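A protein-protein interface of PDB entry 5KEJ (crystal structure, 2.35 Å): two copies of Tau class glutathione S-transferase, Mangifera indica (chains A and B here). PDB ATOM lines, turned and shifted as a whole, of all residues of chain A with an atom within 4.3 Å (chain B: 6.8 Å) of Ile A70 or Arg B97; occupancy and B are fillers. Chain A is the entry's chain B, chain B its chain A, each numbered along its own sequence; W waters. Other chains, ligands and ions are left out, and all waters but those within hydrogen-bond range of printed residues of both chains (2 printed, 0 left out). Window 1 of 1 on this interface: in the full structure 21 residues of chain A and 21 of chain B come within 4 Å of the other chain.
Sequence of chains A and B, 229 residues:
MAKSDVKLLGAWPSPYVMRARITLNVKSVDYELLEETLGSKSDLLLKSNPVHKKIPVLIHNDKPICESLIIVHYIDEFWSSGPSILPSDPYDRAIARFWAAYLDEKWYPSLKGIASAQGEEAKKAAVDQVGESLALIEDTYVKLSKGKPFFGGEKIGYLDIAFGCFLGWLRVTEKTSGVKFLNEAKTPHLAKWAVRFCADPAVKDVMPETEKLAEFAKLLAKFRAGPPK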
ATOM      1  N   ILE A  65       0.125 -15.991  -4.372  1.00  0.00           N
ATOM      2  CA  ILE A  65       0.120 -15.679  -2.942  1.00  0.00           C
ATOM      3  C   ILE A  65      -0.741 -14.430  -2.739  1.00  0.00           C
ATOM      4  O   ILE A  65      -0.448 -13.383  -3.326  1.00  0.00           O
ATOM      5  CB  ILE A  65       1.559 -15.444  -2.396  1.00  0.00           C
ATOM      6  CG1 ILE A  65       2.445 -16.681  -2.621  1.00  0.00           C
ATOM      7  CG2 ILE A  65       1.536 -15.090  -0.930  1.00  0.00           C
ATOM      8  CD1 ILE A  65       3.239 -16.645  -3.919  1.00  0.00           C
ATOM      9  N   CYS A  66      -1.809 -14.544  -1.943  1.00  0.00           N
ATOM     10  CA  CYS A  66      -2.721 -13.412  -1.666  1.00  0.00           C
ATOM     11  C   CYS A  66      -2.570 -12.849  -0.247  1.00  0.00           C
ATOM     12  O   CYS A  66      -2.018 -13.519   0.624  1.00  0.00           O
ATOM     13  CB  CYS A  66      -4.185 -13.827  -1.895  1.00  0.00           C
ATOM     14  SG  CYS A  66      -4.442 -14.779  -3.444  1.00  0.00           S
ATOM     15  N   GLU A  67      -3.083 -11.623  -0.054  1.00  0.00           N
ATOM     16  CA  GLU A  67      -3.085 -10.852   1.207  1.00  0.00           C
ATOM     17  C   GLU A  67      -1.742 -10.185   1.476  1.00  0.00           C
ATOM     18  O   GLU A  67      -0.718 -10.859   1.631  1.00  0.00           O
ATOM     19  CB  GLU A  67      -3.496 -11.715   2.395  1.00  0.00           C
ATOM     20  CG  GLU A  67      -4.900 -12.282   2.256  1.00  0.00           C
ATOM     21  CD  GLU A  67      -5.979 -11.264   2.606  1.00  0.00           C
ATOM     22  OE1 GLU A  67      -6.965 -11.129   1.838  1.00  0.00           O
ATOM     23  OE2 GLU A  67      -5.836 -10.613   3.659  1.00  0.00           O
ATOM     24  N   SER A  68      -1.766  -8.851   1.534  1.00  0.00           N
ATOM     25  CA  SER A  68      -0.550  -8.048   1.490  1.00  0.00           C
ATOM     26  C   SER A  68       0.475  -8.422   2.565  1.00  0.00           C
ATOM     27  O   SER A  68       1.662  -8.549   2.264  1.00  0.00           O
ATOM     28  CB  SER A  68      -0.893  -6.539   1.570  1.00  0.00           C
ATOM     29  OG  SER A  68      -1.567  -6.165   2.762  1.00  0.00           O
ATOM     30  N   LEU A  69       0.059  -8.627   3.804  1.00  0.00           N
ATOM     31  CA  LEU A  69       1.070  -8.901   4.830  1.00  0.00           C
ATOM     32  C   LEU A  69       1.574 -10.354   4.727  1.00  0.00           C
ATOM     33  O   LEU A  69       2.661 -10.687   5.199  1.00  0.00           O
ATOM     34  CB  LEU A  69       0.528  -8.618   6.234  1.00  0.00           C
ATOM     35  CG  LEU A  69       0.154  -7.188   6.637  1.00  0.00           C
ATOM     36  CD1 LEU A  69      -0.320  -7.190   8.067  1.00  0.00           C
ATOM     37  CD2 LEU A  69       1.299  -6.175   6.448  1.00  0.00           C
ATOM     38  N   ILE A  70       0.781 -11.218   4.106  1.00  0.00           N
ATOM     39  CA  ILE A  70       1.214 -12.584   3.882  1.00  0.00           C
ATOM     40  C   ILE A  70       2.237 -12.596   2.753  1.00  0.00           C
ATOM     41  O   ILE A  70       3.214 -13.332   2.800  1.00  0.00           O
ATOM     42  CB  ILE A  70       0.028 -13.518   3.558  1.00  0.00           C
ATOM     43  CG1 ILE A  70      -0.783 -13.785   4.834  1.00  0.00           C
ATOM     44  CG2 ILE A  70       0.542 -14.877   3.006  1.00  0.00           C
ATOM     45  CD1 ILE A  70      -2.152 -14.396   4.574  1.00  0.00           C
ATOM     46  N   ILE A  71       2.002 -11.752   1.756  1.00  0.00           N
ATOM     47  CA  ILE A  71       2.912 -11.564   0.641  1.00  0.00           C
ATOM     48  C   ILE A  71       4.260 -11.053   1.146  1.00  0.00           C
ATOM     49  O   ILE A  71       5.312 -11.546   0.738  1.00  0.00           O
ATOM     50  CB  ILE A  71       2.284 -10.587  -0.407  1.00  0.00           C
ATOM     51  CG1 ILE A  71       1.137 -11.284  -1.135  1.00  0.00           C
ATOM     52  CG2 ILE A  71       3.288 -10.112  -1.413  1.00  0.00           C
ATOM     53  CD1 ILE A  71       0.324 -10.355  -2.013  1.00  0.00           C
ATOM     54  N   VAL A  72       4.229 -10.094   2.068  1.00  0.00           N
ATOM     55  CA  VAL A  72       5.459  -9.520   2.601  1.00  0.00           C
ATOM     56  C   VAL A  72       6.247 -10.565   3.358  1.00  0.00           C
ATOM     57  O   VAL A  72       7.469 -10.638   3.238  1.00  0.00           O
ATOM     58  CB  VAL A  72       5.158  -8.274   3.508  1.00  0.00           C
ATOM     59  CG1 VAL A  72       6.369  -7.856   4.297  1.00  0.00           C
ATOM     60  CG2 VAL A  72       4.697  -7.110   2.645  1.00  0.00           C
ATOM     61  N   HIS A  73       5.544 -11.385   4.133  1.00  0.00           N
ATOM     62  CA  HIS A  73       6.171 -12.488   4.829  1.00  0.00           C
ATOM     63  C   HIS A  73       6.791 -13.442   3.817  1.00  0.00           C
ATOM     64  O   HIS A  73       7.928 -13.849   3.985  1.00  0.00           O
ATOM     65  CB  HIS A  73       5.158 -13.238   5.721  1.00  0.00           C
ATOM     66  CG  HIS A  73       5.030 -12.681   7.107  1.00  0.00           C
ATOM     67  ND1 HIS A  73       4.332 -11.520   7.391  1.00  0.00           N
ATOM     68  CD2 HIS A  73       5.515 -13.128   8.291  1.00  0.00           C
ATOM     69  CE1 HIS A  73       4.388 -11.287   8.694  1.00  0.00           C
ATOM     70  NE2 HIS A  73       5.112 -12.239   9.260  1.00  0.00           N
ATOM     71  N   TYR A  74       6.046 -13.786   2.763  1.00  0.00           N
ATOM     72  CA  TYR A  74       6.534 -14.734   1.757  1.00  0.00           C
ATOM     73  C   TYR A  74       7.807 -14.225   1.096  1.00  0.00           C
ATOM     74  O   TYR A  74       8.785 -14.947   0.990  1.00  0.00           O
ATOM     75  CB  TYR A  74       5.462 -15.006   0.684  1.00  0.00           C
ATOM     76  CG  TYR A  74       5.964 -15.873  -0.451  1.00  0.00           C
ATOM     77  CD1 TYR A  74       5.969 -17.257  -0.341  1.00  0.00           C
ATOM     78  CD2 TYR A  74       6.447 -15.308  -1.630  1.00  0.00           C
ATOM     79  CE1 TYR A  74       6.441 -18.063  -1.374  1.00  0.00           C
ATOM     80  CE2 TYR A  74       6.913 -16.106  -2.681  1.00  0.00           C
ATOM     81  CZ  TYR A  74       6.905 -17.486  -2.538  1.00  0.00           C
ATOM     82  OH  TYR A  74       7.356 -18.293  -3.551  1.00  0.00           O
ATOM     83  N   GLU A  77      10.676 -14.368   3.492  1.00  0.00           N
ATOM     84  CA  GLU A  77      11.087 -15.731   3.803  1.00  0.00           C
ATOM     85  C   GLU A  77      11.686 -16.463   2.610  1.00  0.00           C
ATOM     86  O   GLU A  77      12.593 -17.280   2.771  1.00  0.00           O
ATOM     87  CB  GLU A  77       9.904 -16.509   4.361  1.00  0.00           C
ATOM     88  CG  GLU A  77       9.547 -16.067   5.787  1.00  0.00           C
ATOM     89  CD  GLU A  77       8.250 -16.670   6.272  1.00  0.00           C
ATOM     90  OE1 GLU A  77       7.678 -17.513   5.550  1.00  0.00           O
ATOM     91  OE2 GLU A  77       7.791 -16.283   7.373  1.00  0.00           O
ATOM     92  N   LEU B  69      -2.891 -15.615  16.863  1.00  0.00           N
ATOM     93  CA  LEU B  69      -2.033 -16.107  15.782  1.00  0.00           C
ATOM     94  C   LEU B  69      -0.602 -15.549  15.868  1.00  0.00           C
ATOM     95  O   LEU B  69       0.364 -16.207  15.462  1.00  0.00           O
ATOM     96  CB  LEU B  69      -2.656 -15.779  14.420  1.00  0.00           C
ATOM     97  CG  LEU B  69      -4.025 -16.414  14.147  1.00  0.00           C
ATOM     98  CD1 LEU B  69      -4.491 -16.054  12.752  1.00  0.00           C
ATOM     99  CD2 LEU B  69      -3.962 -17.933  14.307  1.00  0.00           C
ATOM    100  N   HIS B  73       2.661 -18.079  16.324  1.00  0.00           N
ATOM    101  CA  HIS B  73       3.928 -17.817  15.639  1.00  0.00           C
ATOM    102  C   HIS B  73       5.096 -17.690  16.616  1.00  0.00           C
ATOM    103  O   HIS B  73       6.145 -18.286  16.397  1.00  0.00           O
ATOM    104  CB  HIS B  73       3.850 -16.533  14.805  1.00  0.00           C
ATOM    105  CG  HIS B  73       3.272 -16.719  13.435  1.00  0.00           C
ATOM    106  ND1 HIS B  73       1.923 -16.892  13.211  1.00  0.00           N
ATOM    107  CD2 HIS B  73       3.860 -16.715  12.216  1.00  0.00           C
ATOM    108  CE1 HIS B  73       1.708 -17.013  11.912  1.00  0.00           C
ATOM    109  NE2 HIS B  73       2.868 -16.904  11.285  1.00  0.00           N
ATOM    110  N   GLU B  77       8.330 -19.817  16.757  1.00  0.00           N
ATOM    111  CA  GLU B  77       9.641 -19.262  16.452  1.00  0.00           C
ATOM    112  C   GLU B  77      10.591 -19.308  17.662  1.00  0.00           C
ATOM    113  O   GLU B  77      11.803 -19.405  17.474  1.00  0.00           O
ATOM    114  CB  GLU B  77       9.526 -17.836  15.925  1.00  0.00           C
ATOM    115  CG  GLU B  77       8.997 -17.746  14.483  1.00  0.00           C
ATOM    116  CD  GLU B  77       8.562 -16.343  14.122  1.00  0.00           C
ATOM    117  OE1 GLU B  77       8.676 -15.459  14.990  1.00  0.00           O
ATOM    118  OE2 GLU B  77       8.106 -16.119  12.979  1.00  0.00           O
ATOM    119  N   LEU B  86       4.345 -24.128  12.064  1.00  0.00           N
ATOM    120  CA  LEU B  86       4.175 -23.606  10.710  1.00  0.00           C
ATOM    121  C   LEU B  86       4.844 -24.582   9.752  1.00  0.00           C
ATOM    122  O   LEU B  86       5.820 -25.242  10.134  1.00  0.00           O
ATOM    123  CB  LEU B  86       4.773 -22.198  10.573  1.00  0.00           C
ATOM    124  CG  LEU B  86       3.983 -20.914  10.916  1.00  0.00           C
ATOM    125  CD1 LEU B  86       2.707 -20.752  10.065  1.00  0.00           C
ATOM    126  CD2 LEU B  86       3.652 -20.820  12.389  1.00  0.00           C
ATOM    127  N   PRO B  87       4.315 -24.697   8.520  1.00  0.00           N
ATOM    128  CA  PRO B  87       4.926 -25.574   7.514  1.00  0.00           C
ATOM    129  C   PRO B  87       6.369 -25.172   7.243  1.00  0.00           C
ATOM    130  O   PRO B  87       6.721 -24.024   7.490  1.00  0.00           O
ATOM    131  CB  PRO B  87       4.048 -25.363   6.270  1.00  0.00           C
ATOM    132  CG  PRO B  87       2.724 -24.963   6.830  1.00  0.00           C
ATOM    133  CD  PRO B  87       3.052 -24.109   8.041  1.00  0.00           C
ATOM    134  N   PRO B  90       8.107 -21.919   2.537  1.00  0.00           N
ATOM    135  CA  PRO B  90       7.529 -20.565   2.539  1.00  0.00           C
ATOM    136  C   PRO B  90       6.181 -20.478   1.828  1.00  0.00           C
ATOM    137  O   PRO B  90       5.279 -19.772   2.318  1.00  0.00           O
ATOM    138  CB  PRO B  90       8.575 -19.722   1.788  1.00  0.00           C
ATOM    139  CG  PRO B  90       9.850 -20.441   1.988  1.00  0.00           C
ATOM    140  CD  PRO B  90       9.524 -21.910   2.139  1.00  0.00           C
ATOM    141  N   ASP B  92       4.031 -22.941   1.364  1.00  0.00           N
ATOM    142  CA  ASP B  92       3.079 -23.633   2.216  1.00  0.00           C
ATOM    143  C   ASP B  92       2.722 -22.787   3.453  1.00  0.00           C
ATOM    144  O   ASP B  92       1.584 -22.837   3.926  1.00  0.00           O
ATOM    145  CB  ASP B  92       3.632 -25.000   2.643  1.00  0.00           C
ATOM    146  CG  ASP B  92       3.620 -26.038   1.491  1.00  0.00           C
ATOM    147  OD1 ASP B  92       2.913 -25.831   0.479  1.00  0.00           O
ATOM    148  OD2 ASP B  92       4.316 -27.065   1.597  1.00  0.00           O
ATOM    149  N   ARG B  93       3.684 -22.020   3.977  1.00  0.00           N
ATOM    150  CA  ARG B  93       3.412 -21.174   5.137  1.00  0.00           C
ATOM    151  C   ARG B  93       2.397 -20.098   4.764  1.00  0.00           C
ATOM    152  O   ARG B  93       1.493 -19.820   5.535  1.00  0.00           O
ATOM    153  CB  ARG B  93       4.688 -20.530   5.694  1.00  0.00           C
ATOM    154  CG  ARG B  93       5.429 -21.444   6.660  1.00  0.00           C
ATOM    155  CD  ARG B  93       6.390 -20.700   7.607  1.00  0.00           C
ATOM    156  NE  ARG B  93       7.394 -19.959   6.856  1.00  0.00           N
ATOM    157  CZ  ARG B  93       8.493 -20.504   6.354  1.00  0.00           C
ATOM    158  NH1 ARG B  93       9.351 -19.759   5.672  1.00  0.00           N
ATOM    159  NH2 ARG B  93       8.734 -21.793   6.536  1.00  0.00           N
ATOM    160  N   ALA B  94       2.550 -19.534   3.570  1.00  0.00           N
ATOM    161  CA  ALA B  94       1.621 -18.552   3.008  1.00  0.00           C
ATOM    162  C   ALA B  94       0.199 -19.082   2.848  1.00  0.00           C
ATOM    163  O   ALA B  94      -0.770 -18.357   3.117  1.00  0.00           O
ATOM    164  CB  ALA B  94       2.124 -18.072   1.665  1.00  0.00           C
ATOM    165  N   ILE B  95       0.073 -20.331   2.388  1.00  0.00           N
ATOM    166  CA  ILE B  95      -1.234 -20.959   2.223  1.00  0.00           C
ATOM    167  C   ILE B  95      -1.909 -21.108   3.582  1.00  0.00           C
ATOM    168  O   ILE B  95      -3.091 -20.794   3.762  1.00  0.00           O
ATOM    169  CB  ILE B  95      -1.120 -22.341   1.539  1.00  0.00           C
ATOM    170  CG1 ILE B  95      -0.683 -22.184   0.086  1.00  0.00           C
ATOM    171  CG2 ILE B  95      -2.433 -23.087   1.580  1.00  0.00           C
ATOM    172  CD1 ILE B  95      -1.632 -21.384  -0.735  1.00  0.00           C
ATOM    173  N   ALA B  96      -1.127 -21.559   4.544  1.00  0.00           N
ATOM    174  CA  ALA B  96      -1.609 -21.837   5.875  1.00  0.00           C
ATOM    175  C   ALA B  96      -2.045 -20.549   6.590  1.00  0.00           C
ATOM    176  O   ALA B  96      -3.086 -20.527   7.250  1.00  0.00           O
ATOM    177  CB  ALA B  96      -0.517 -22.564   6.681  1.00  0.00           C
ATOM    178  N   ARG B  97      -1.223 -19.501   6.485  1.00  0.00           N
ATOM    179  CA  ARG B  97      -1.538 -18.176   7.025  1.00  0.00           C
ATOM    180  C   ARG B  97      -2.786 -17.619   6.375  1.00  0.00           C
ATOM    181  O   ARG B  97      -3.652 -17.056   7.048  1.00  0.00           O
ATOM    182  CB  ARG B  97      -0.362 -17.207   6.819  1.00  0.00           C
ATOM    183  CG  ARG B  97       0.788 -17.468   7.769  1.00  0.00           C
ATOM    184  CD  ARG B  97       1.978 -16.576   7.495  1.00  0.00           C
ATOM    185  NE  ARG B  97       3.077 -16.894   8.408  1.00  0.00           N
ATOM    186  CZ  ARG B  97       4.360 -16.877   8.071  1.00  0.00           C
ATOM    187  NH1 ARG B  97       5.285 -17.184   8.963  1.00  0.00           N
ATOM    188  NH2 ARG B  97       4.725 -16.561   6.845  1.00  0.00           N
ATOM    189  N   PHE B  98      -2.869 -17.772   5.057  1.00  0.00           N
ATOM    190  CA  PHE B  98      -4.031 -17.315   4.303  1.00  0.00           C
ATOM    191  C   PHE B  98      -5.317 -17.900   4.840  1.00  0.00           C
ATOM    192  O   PHE B  98      -6.278 -17.172   5.075  1.00  0.00           O
ATOM    193  CB  PHE B  98      -3.885 -17.676   2.825  1.00  0.00           C
ATOM    194  CG  PHE B  98      -5.082 -17.309   1.986  1.00  0.00           C
ATOM    195  CD1 PHE B  98      -5.175 -16.055   1.399  1.00  0.00           C
ATOM    196  CD2 PHE B  98      -6.111 -18.224   1.774  1.00  0.00           C
ATOM    197  CE1 PHE B  98      -6.271 -15.714   0.628  1.00  0.00           C
ATOM    198  CE2 PHE B  98      -7.220 -17.881   1.006  1.00  0.00           C
ATOM    199  CZ  PHE B  98      -7.295 -16.622   0.432  1.00  0.00           C
ATOM    200  N   TRP B  99      -5.350 -19.217   5.031  1.00  0.00           N
ATOM    201  CA  TRP B  99      -6.600 -19.829   5.431  1.00  0.00           C
ATOM    202  C   TRP B  99      -6.918 -19.514   6.892  1.00  0.00           C
ATOM    203  O   TRP B  99      -8.079 -19.317   7.229  1.00  0.00           O
ATOM    204  CB  TRP B  99      -6.571 -21.329   5.149  1.00  0.00           C
ATOM    205  CG  TRP B  99      -6.772 -21.598   3.670  1.00  0.00           C
ATOM    206  CD1 TRP B  99      -5.835 -22.035   2.771  1.00  0.00           C
ATOM    207  CD2 TRP B  99      -7.981 -21.389   2.922  1.00  0.00           C
ATOM    208  NE1 TRP B  99      -6.393 -22.124   1.513  1.00  0.00           N
ATOM    209  CE2 TRP B  99      -7.708 -21.740   1.578  1.00  0.00           C
ATOM    210  CE3 TRP B  99      -9.268 -20.937   3.260  1.00  0.00           C
ATOM    211  CZ2 TRP B  99      -8.679 -21.662   0.569  1.00  0.00           C
ATOM    212  CZ3 TRP B  99     -10.232 -20.863   2.259  1.00  0.00           C
ATOM    213  CH2 TRP B  99      -9.931 -21.227   0.931  1.00  0.00           C
ATOM    214  N   ALA B 100      -5.907 -19.417   7.754  1.00  0.00           N
ATOM    215  CA  ALA B 100      -6.155 -18.945   9.123  1.00  0.00           C
ATOM    216  C   ALA B 100      -6.750 -17.526   9.112  1.00  0.00           C
ATOM    217  O   ALA B 100      -7.664 -17.220   9.885  1.00  0.00           O
ATOM    218  CB  ALA B 100      -4.878 -18.972   9.946  1.00  0.00           C
ATOM    219  N   ALA B 101      -6.249 -16.659   8.233  1.00  0.00           N
ATOM    220  CA  ALA B 101      -6.764 -15.287   8.184  1.00  0.00           C
ATOM    221  C   ALA B 101      -8.203 -15.282   7.684  1.00  0.00           C
ATOM    222  O   ALA B 101      -9.026 -14.524   8.166  1.00  0.00           O
ATOM    223  CB  ALA B 101      -5.885 -14.397   7.300  1.00  0.00           C
ATOM    224  N   TYR B 102      -8.505 -16.163   6.736  1.00  0.00           N
ATOM    225  CA  TYR B 102      -9.860 -16.291   6.204  1.00  0.00           C
ATOM    226  C   TYR B 102     -10.839 -16.760   7.274  1.00  0.00           C
ATOM    227  O   TYR B 102     -12.009 -16.371   7.258  1.00  0.00           O
ATOM    228  CB  TYR B 102      -9.863 -17.259   5.019  1.00  0.00           C
ATOM    229  CG  TYR B 102     -11.234 -17.676   4.558  1.00  0.00           C
ATOM    230  CD1 TYR B 102     -11.919 -16.940   3.601  1.00  0.00           C
ATOM    231  CD2 TYR B 102     -11.850 -18.810   5.079  1.00  0.00           C
ATOM    232  CE1 TYR B 102     -13.184 -17.317   3.178  1.00  0.00           C
ATOM    233  CE2 TYR B 102     -13.110 -19.201   4.655  1.00  0.00           C
ATOM    234  CZ  TYR B 102     -13.767 -18.448   3.707  1.00  0.00           C
ATOM    235  OH  TYR B 102     -15.013 -18.833   3.286  1.00  0.00           O
ATOM    236  N   TYR B 158      -0.318 -25.424  12.179  1.00  0.00           N
ATOM    237  CA  TYR B 158      -0.907 -24.101  12.237  1.00  0.00           C
ATOM    238  C   TYR B 158      -2.399 -24.059  11.880  1.00  0.00           C
ATOM    239  O   TYR B 158      -3.250 -23.670  12.695  1.00  0.00           O
ATOM    240  CB  TYR B 158      -0.123 -23.190  11.287  1.00  0.00           C
ATOM    241  CG  TYR B 158      -0.483 -21.725  11.387  1.00  0.00           C
ATOM    242  CD1 TYR B 158      -0.047 -20.955  12.456  1.00  0.00           C
ATOM    243  CD2 TYR B 158      -1.259 -21.113  10.411  1.00  0.00           C
ATOM    244  CE1 TYR B 158      -0.370 -19.609  12.538  1.00  0.00           C
ATOM    245  CE2 TYR B 158      -1.581 -19.776  10.485  1.00  0.00           C
ATOM    246  CZ  TYR B 158      -1.142 -19.026  11.552  1.00  0.00           C
ATOM    247  OH  TYR B 158      -1.470 -17.683  11.636  1.00  0.00           O
ATOM    248  N   LEU B 159      -2.713 -24.478  10.661  1.00  0.00           N
ATOM    249  CA  LEU B 159      -4.079 -24.428  10.157  1.00  0.00           C
ATOM    250  C   LEU B 159      -5.016 -25.332  10.951  1.00  0.00           C
ATOM    251  O   LEU B 159      -6.180 -24.962  11.183  1.00  0.00           O
ATOM    252  CB  LEU B 159      -4.110 -24.807   8.667  1.00  0.00           C
ATOM    253  CG  LEU B 159      -5.418 -24.489   7.957  1.00  0.00           C
ATOM    254  CD1 LEU B 159      -5.869 -23.044   8.324  1.00  0.00           C
ATOM    255  CD2 LEU B 159      -5.217 -24.614   6.468  1.00  0.00           C
HETATM  256  O   HOH W   1       3.515 -15.795   4.050  1.00  0.00           O
HETATM  257  O   HOH W   2       5.791 -17.298   3.595  1.00  0.00           O
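NE of Arg B93 is in salt-bridge range of OE1 of Glu A77 (2.8 Å). The guanidinium group of Arg B97 lies within salt-bridge range of the side-chain carboxylate of Glu A77 (3.1 Å).
The backbone carbonyl oxygen (O) of Pro B87 sits close to the guanidinium group (NH2) of Arg B93, at 3.2 Å. A ring nitrogen (NE2) of His B73 is in hydrogen-bond range of the guanidinium group of Arg B97, 2.9 Å away. The backbone carbonyl oxygen of Leu A69 sits at hydrogen-bond distance from a ring nitrogen (ND1) of His A73.
Ile A65 touches Ala B94. Phe B98 touches Cys A66 (CE1 to CB, 3.8 Å). CD1 of Phe B98 touches CG of Glu A67 (3.9 Å). Ala B94 touches Ile A70 (O to CG2, 3.7 Å). Arg B97 touches Ile A70 (C to CD1, 3.7 Å). Ile A70 touches Phe B98. NH2 of Arg B97 touches CB of His A73 (3.5 Å). CD1 of Tyr A74 touches O of Pro B90 (3.7 Å).
Of the printed residues of chain B, Ile A70 touches Ala B94, Arg B97 and Phe B98. Arg B97 touches three residues of chain A. Printed residues of chain B within 4 Å of Glu A77: Arg B93 (2.8 Å) and Arg B97 (3.1 Å). Printed residues of chain B within 4 Å of Glu A67: Phe B98 (3.9 Å). Of the printed residues of chain B, Tyr A74 touches Pro B90 (3.7 Å). Printed residues of chain A within 4 Å of Ala B94: Ile A65 and Ile A70. Of the printed residues of chain A, Pro B90 touches Tyr A74 (3.7 Å). Tyr B102 touches none of the printed residues of chain A. Leu B86 touches none of the printed residues of chain A. The nearest printed residue of chain B that does not touch Glu A77 is Pro B90 (4.3 Å).
Of the 11 printed residues of chain A, 7 touch a printed residue of chain B. Hydrophobic or aromatic side chains of chain A that line the printed part of chain B: Ile A65, Ile A70, His A73 and Tyr A74. Hydrophobic or aromatic side chains of chain B within 4 Å of the printed part of chain A: Ala B94 and Phe B98. Among the printed residues, 10 pairs touch across the chains. Among the printed residues, Asp or Glu carboxylates within 4 Å of a Lys or Arg side-chain nitrogen of the other chain: Glu A77 with Arg B93 (2.8 Å) and Glu A77 with Arg B97 (3.1 Å).
3 positions are printed for both chains.
Water W2 lies within hydrogen-bond range of OE1 of Glu A77 (2.7 Å), O of Pro B90 (2.8 Å) and NH2 of Arg B97 (3.5 Å). Water W1 lies within hydrogen-bond range of the backbone carbonyl oxygen (O) of Ile A70 (2.8 Å), the guanidinium group (NH2) of Arg B97 (3.1 Å) and the backbone NH (N) of Tyr A74 (3.5 Å).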
